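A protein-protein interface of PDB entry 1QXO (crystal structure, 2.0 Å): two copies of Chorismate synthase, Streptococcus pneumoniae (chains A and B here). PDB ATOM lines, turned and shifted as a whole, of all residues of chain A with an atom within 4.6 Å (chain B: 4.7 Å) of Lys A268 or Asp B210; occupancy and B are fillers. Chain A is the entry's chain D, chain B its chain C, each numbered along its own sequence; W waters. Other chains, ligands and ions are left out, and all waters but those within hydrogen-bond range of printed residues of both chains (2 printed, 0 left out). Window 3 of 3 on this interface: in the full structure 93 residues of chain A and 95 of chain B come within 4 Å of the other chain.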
ATOM      1  N   ARG A 267      20.047  -4.448  16.890  1.00  0.00           N
ATOM      2  CA  ARG A 267      19.414  -5.715  16.534  1.00  0.00           C
ATOM      3  C   ARG A 267      20.031  -6.381  15.302  1.00  0.00           C
ATOM      4  O   ARG A 267      20.887  -5.828  14.613  1.00  0.00           O
ATOM      5  CB  ARG A 267      17.940  -5.487  16.227  1.00  0.00           C
ATOM      6  CG  ARG A 267      17.130  -5.048  17.444  1.00  0.00           C
ATOM      7  CD  ARG A 267      15.691  -5.179  16.996  1.00  0.00           C
ATOM      8  NE  ARG A 267      14.678  -4.746  17.937  1.00  0.00           N
ATOM      9  CZ  ARG A 267      13.397  -5.054  17.675  1.00  0.00           C
ATOM     10  NH1 ARG A 267      13.080  -5.748  16.579  1.00  0.00           N
ATOM     11  NH2 ARG A 267      12.430  -4.680  18.501  1.00  0.00           N
ATOM     12  N   LYS A 268      19.567  -7.599  15.034  1.00  0.00           N
ATOM     13  CA  LYS A 268      20.052  -8.347  13.888  1.00  0.00           C
ATOM     14  C   LYS A 268      19.192  -8.125  12.646  1.00  0.00           C
ATOM     15  O   LYS A 268      18.026  -7.823  12.797  1.00  0.00           O
ATOM     16  CB  LYS A 268      20.076  -9.849  14.197  1.00  0.00           C
ATOM     17  CG  LYS A 268      21.133 -10.123  15.286  1.00  0.00           C
ATOM     18  CD  LYS A 268      20.823 -11.414  16.037  1.00  0.00           C
ATOM     19  CE  LYS A 268      21.148 -12.630  15.208  1.00  0.00           C
ATOM     20  NZ  LYS A 268      22.565 -13.065  15.301  1.00  0.00           N
ATOM     21  N   GLY A 269      19.778  -8.317  11.498  1.00  0.00           N
ATOM     22  CA  GLY A 269      19.113  -8.222  10.217  1.00  0.00           C
ATOM     23  C   GLY A 269      17.765  -8.930  10.265  1.00  0.00           C
ATOM     24  O   GLY A 269      16.762  -8.336   9.902  1.00  0.00           O
ATOM     25  N   SER A 270      17.741 -10.179  10.737  1.00  0.00           N
ATOM     26  CA  SER A 270      16.462 -10.898  10.740  1.00  0.00           C
ATOM     27  C   SER A 270      15.465 -10.271  11.678  1.00  0.00           C
ATOM     28  O   SER A 270      14.279 -10.575  11.574  1.00  0.00           O
ATOM     29  CB  SER A 270      16.703 -12.375  11.137  1.00  0.00           C
ATOM     30  OG  SER A 270      17.504 -12.302  12.296  1.00  0.00           O
ATOM     31  N   GLN A 271      15.902  -9.421  12.612  1.00  0.00           N
ATOM     32  CA  GLN A 271      14.899  -8.823  13.502  1.00  0.00           C
ATOM     33  C   GLN A 271      14.418  -7.508  12.920  1.00  0.00           C
ATOM     34  O   GLN A 271      13.540  -6.914  13.524  1.00  0.00           O
ATOM     35  CB  GLN A 271      15.455  -8.622  14.916  1.00  0.00           C
ATOM     36  CG  GLN A 271      15.926  -9.875  15.634  1.00  0.00           C
ATOM     37  CD  GLN A 271      16.812  -9.721  16.840  1.00  0.00           C
ATOM     38  OE1 GLN A 271      17.529  -8.741  17.088  1.00  0.00           O
ATOM     39  NE2 GLN A 271      16.808 -10.742  17.708  1.00  0.00           N
ATOM     40  N   VAL A 272      14.965  -6.991  11.848  1.00  0.00           N
ATOM     41  CA  VAL A 272      14.638  -5.681  11.296  1.00  0.00           C
ATOM     42  C   VAL A 272      13.963  -5.652   9.931  1.00  0.00           C
ATOM     43  O   VAL A 272      13.068  -4.786   9.764  1.00  0.00           O
ATOM     44  CB  VAL A 272      15.927  -4.808  11.243  1.00  0.00           C
ATOM     45  CG1 VAL A 272      15.760  -3.429  10.607  1.00  0.00           C
ATOM     46  CG2 VAL A 272      16.545  -4.616  12.621  1.00  0.00           C
ATOM     47  N   GLN B 206      30.190 -14.764  14.365  1.00  0.00           N
ATOM     48  CA  GLN B 206      28.988 -15.460  14.825  1.00  0.00           C
ATOM     49  C   GLN B 206      27.773 -15.106  13.960  1.00  0.00           C
ATOM     50  O   GLN B 206      27.047 -15.907  13.359  1.00  0.00           O
ATOM     51  CB  GLN B 206      28.761 -14.996  16.272  1.00  0.00           C
ATOM     52  CG  GLN B 206      27.773 -15.831  17.078  1.00  0.00           C
ATOM     53  CD  GLN B 206      28.369 -17.207  17.365  1.00  0.00           C
ATOM     54  OE1 GLN B 206      28.155 -18.126  16.564  1.00  0.00           O
ATOM     55  NE2 GLN B 206      29.142 -17.288  18.452  1.00  0.00           N
ATOM     56  N   ILE B 207      27.612 -13.785  13.820  1.00  0.00           N
ATOM     57  CA  ILE B 207      26.539 -13.225  12.987  1.00  0.00           C
ATOM     58  C   ILE B 207      26.581 -13.858  11.610  1.00  0.00           C
ATOM     59  O   ILE B 207      25.576 -14.281  11.037  1.00  0.00           O
ATOM     60  CB  ILE B 207      26.678 -11.690  12.885  1.00  0.00           C
ATOM     61  CG1 ILE B 207      26.313 -11.034  14.221  1.00  0.00           C
ATOM     62  CG2 ILE B 207      25.878 -11.133  11.729  1.00  0.00           C
ATOM     63  CD1 ILE B 207      24.866 -11.260  14.636  1.00  0.00           C
ATOM     64  N   LYS B 208      27.781 -13.905  11.048  1.00  0.00           N
ATOM     65  CA  LYS B 208      27.957 -14.466   9.718  1.00  0.00           C
ATOM     66  C   LYS B 208      27.608 -15.960   9.741  1.00  0.00           C
ATOM     67  O   LYS B 208      26.823 -16.402   8.905  1.00  0.00           O
ATOM     68  CB  LYS B 208      29.384 -14.243   9.252  1.00  0.00           C
ATOM     69  CG  LYS B 208      29.739 -14.875   7.930  1.00  0.00           C
ATOM     70  CD  LYS B 208      31.166 -14.513   7.519  1.00  0.00           C
ATOM     71  CE  LYS B 208      31.484 -14.969   6.102  1.00  0.00           C
ATOM     72  NZ  LYS B 208      32.948 -15.071   5.848  1.00  0.00           N
ATOM     73  N   ARG B 209      28.147 -16.676  10.750  1.00  0.00           N
ATOM     74  CA  ARG B 209      27.757 -18.095  10.744  1.00  0.00           C
ATOM     75  C   ARG B 209      26.230 -18.078  10.893  1.00  0.00           C
ATOM     76  O   ARG B 209      25.587 -18.556   9.969  1.00  0.00           O
ATOM     77  CB  ARG B 209      28.440 -19.066  11.627  1.00  0.00           C
ATOM     78  CG  ARG B 209      28.769 -18.899  13.069  1.00  0.00           C
ATOM     79  CD  ARG B 209      30.077 -19.674  13.388  1.00  0.00           C
ATOM     80  NE  ARG B 209      30.676 -18.944  14.494  1.00  0.00           N
ATOM     81  CZ  ARG B 209      31.896 -18.468  14.624  1.00  0.00           C
ATOM     82  NH1 ARG B 209      32.863 -18.594  13.744  1.00  0.00           N
ATOM     83  NH2 ARG B 209      32.125 -17.820  15.753  1.00  0.00           N
ATOM     84  N   ASP B 210      25.702 -17.482  11.952  1.00  0.00           N
ATOM     85  CA  ASP B 210      24.257 -17.458  12.085  1.00  0.00           C
ATOM     86  C   ASP B 210      23.488 -17.077  10.837  1.00  0.00           C
ATOM     87  O   ASP B 210      22.244 -17.123  10.921  1.00  0.00           O
ATOM     88  CB  ASP B 210      23.794 -16.525  13.216  1.00  0.00           C
ATOM     89  CG  ASP B 210      24.251 -17.151  14.518  1.00  0.00           C
ATOM     90  OD1 ASP B 210      24.463 -16.389  15.479  1.00  0.00           O
ATOM     91  OD2 ASP B 210      24.428 -18.381  14.503  1.00  0.00           O
ATOM     92  N   GLY B 211      24.146 -16.610   9.801  1.00  0.00           N
ATOM     93  CA  GLY B 211      23.581 -16.173   8.564  1.00  0.00           C
ATOM     94  C   GLY B 211      22.824 -14.846   8.516  1.00  0.00           C
ATOM     95  O   GLY B 211      21.984 -14.537   7.679  1.00  0.00           O
ATOM     96  N   ASP B 212      23.081 -14.000   9.496  1.00  0.00           N
ATOM     97  CA  ASP B 212      22.358 -12.757   9.718  1.00  0.00           C
ATOM     98  C   ASP B 212      23.238 -11.554   9.444  1.00  0.00           C
ATOM     99  O   ASP B 212      24.313 -11.725   8.855  1.00  0.00           O
ATOM    100  CB  ASP B 212      21.967 -12.841  11.188  1.00  0.00           C
ATOM    101  CG  ASP B 212      20.642 -12.142  11.484  1.00  0.00           C
ATOM    102  OD1 ASP B 212      19.972 -12.713  12.369  1.00  0.00           O
ATOM    103  OD2 ASP B 212      20.364 -11.100  10.853  1.00  0.00           O
ATOM    104  N   THR B 213      22.795 -10.377   9.886  1.00  0.00           N
ATOM    105  CA  THR B 213      23.610  -9.162   9.645  1.00  0.00           C
ATOM    106  C   THR B 213      23.433  -8.271  10.865  1.00  0.00           C
ATOM    107  O   THR B 213      22.506  -8.474  11.660  1.00  0.00           O
ATOM    108  CB  THR B 213      23.194  -8.405   8.373  1.00  0.00           C
ATOM    109  OG1 THR B 213      21.829  -7.980   8.437  1.00  0.00           O
ATOM    110  CG2 THR B 213      23.302  -9.267   7.125  1.00  0.00           C
ATOM    111  N   ILE B 214      24.298  -7.268  11.021  1.00  0.00           N
ATOM    112  CA  ILE B 214      24.185  -6.311  12.116  1.00  0.00           C
ATOM    113  C   ILE B 214      24.602  -4.938  11.569  1.00  0.00           C
ATOM    114  O   ILE B 214      25.374  -4.748  10.637  1.00  0.00           O
ATOM    115  CB  ILE B 214      25.052  -6.664  13.347  1.00  0.00           C
ATOM    116  CG1 ILE B 214      26.506  -6.988  12.929  1.00  0.00           C
ATOM    117  CG2 ILE B 214      24.461  -7.839  14.086  1.00  0.00           C
ATOM    118  CD1 ILE B 214      27.495  -6.929  14.108  1.00  0.00           C
ATOM    119  N   PRO B 312      20.852  -2.959  10.070  1.00  0.00           N
ATOM    120  CA  PRO B 312      21.607  -4.101   9.558  1.00  0.00           C
ATOM    121  C   PRO B 312      21.426  -4.230   8.049  1.00  0.00           C
ATOM    122  O   PRO B 312      20.378  -3.916   7.469  1.00  0.00           O
ATOM    123  CB  PRO B 312      21.080  -5.271  10.348  1.00  0.00           C
ATOM    124  CG  PRO B 312      20.311  -4.679  11.497  1.00  0.00           C
ATOM    125  CD  PRO B 312      19.782  -3.340  11.015  1.00  0.00           C
ATOM    126  N   LYS B 318      20.663 -16.059   4.568  1.00  0.00           N
ATOM    127  CA  LYS B 318      19.540 -16.910   4.994  1.00  0.00           C
ATOM    128  C   LYS B 318      18.336 -16.028   4.704  1.00  0.00           C
ATOM    129  O   LYS B 318      17.915 -15.213   5.514  1.00  0.00           O
ATOM    130  CB  LYS B 318      19.784 -17.216   6.470  1.00  0.00           C
ATOM    131  CG  LYS B 318      21.285 -17.413   6.608  1.00  0.00           C
ATOM    132  CD  LYS B 318      21.905 -18.441   7.497  1.00  0.00           C
ATOM    133  CE  LYS B 318      20.957 -19.507   7.882  1.00  0.00           C
ATOM    134  NZ  LYS B 318      19.792 -18.964   8.674  1.00  0.00           N
HETATM  135  O   HOH W   1      20.342 -15.158  13.894  1.00  0.00           O
HETATM  136  O   HOH W   2      24.356 -14.347  17.168  1.00  0.00           O
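O of Ile B207 lies within hydrogen-bond range of N of Asp B212 (2.9 Å). NH1 of Arg A267 sits at hydrogen-bond distance from O of Gln A271, at 3.3 Å. The backbone NH of Lys A268 is in hydrogen-bond range of the side-chain amide oxygen of Gln A271 (3.1 Å).
Printed residues of chain B within 4 Å of Arg A267: Pro B312 (3.4 Å). Lys A268 touches five residues of chain B. Gln A271 touches none of the printed residues of chain B. Gln B206 touches none of the printed residues of chain A. Printed residues of chain A within 4 Å of Ile B207: Lys A268 (3.0 Å). Of the printed residues of chain A, Asp B210 touches Lys A268 (3.8 Å). Printed residues of chain A within 4 Å of Asp B212: Lys A268 (3.1 Å), Gly A269 (2.9 Å) and Ser A270 (2.5 Å). Printed residues of chain A within 4 Å of Thr B213: Lys A268 and Gly A269. Of the printed residues of chain A, Pro B312 touches Arg A267, Lys A268, Gly A269 and Val A272. The nearest residue of chain B that does not touch Lys A268 is Ile B214 (4.2 Å).
Water W2 bridges the side-chain carboxylate of Asp B210 (2.7 Å) and the side-chain amino group of Lys A268 (2.9 Å). Water W1 bridges OD1 of Asp B212 (2.9 Å) and NZ of Lys A268 (3.4 Å).
No position is printed for both chains.
OD1 of Asp B210 lies within salt-bridge range of NZ of Lys A268. The side-chain carboxylate of Asp B212 is in salt-bridge range of the side-chain amino group of Lys A268, 3.9 Å away. The backbone NH (N) of Gly A269 sits at hydrogen-bond distance from the side-chain carboxylate (OD2) of Asp B212 (2.9 Å). OD1 of Asp B212 lies within hydrogen-bond range of OG of Ser A270, at 2.5 Å. N of Gly A269 lies within hydrogen-bond range of O of Thr B213 (2.7 Å).
Arg A267 touches Pro B312. Lys A268 touches Ile B207 (NZ to CD1, 3.0 Å). CA of Lys A268 touches O of Thr B213, 3.3 Å away. CG of Pro B312 touches C of Lys A268 (3.8 Å). Gly A269 touches Pro B312. Pro B312 touches Val A272.
Printed residues of chain A that touch a printed residue of chain B: Arg A267, Lys A268, Gly A269, Ser A270 and Val A272. Printed residues of chain B that touch a printed residue of chain A: Ile B207, Asp B210, Asp B212, Thr B213 and Pro B312. Among the printed residues, 11 pairs touch across the chains. Among the printed residues, Asp or Glu carboxylates within 4 Å of a Lys or Arg side-chain nitrogen of the other chain: Lys A268 with Asp B210 (3.8 Å) and Lys A268 with Asp B212 (3.9 Å).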
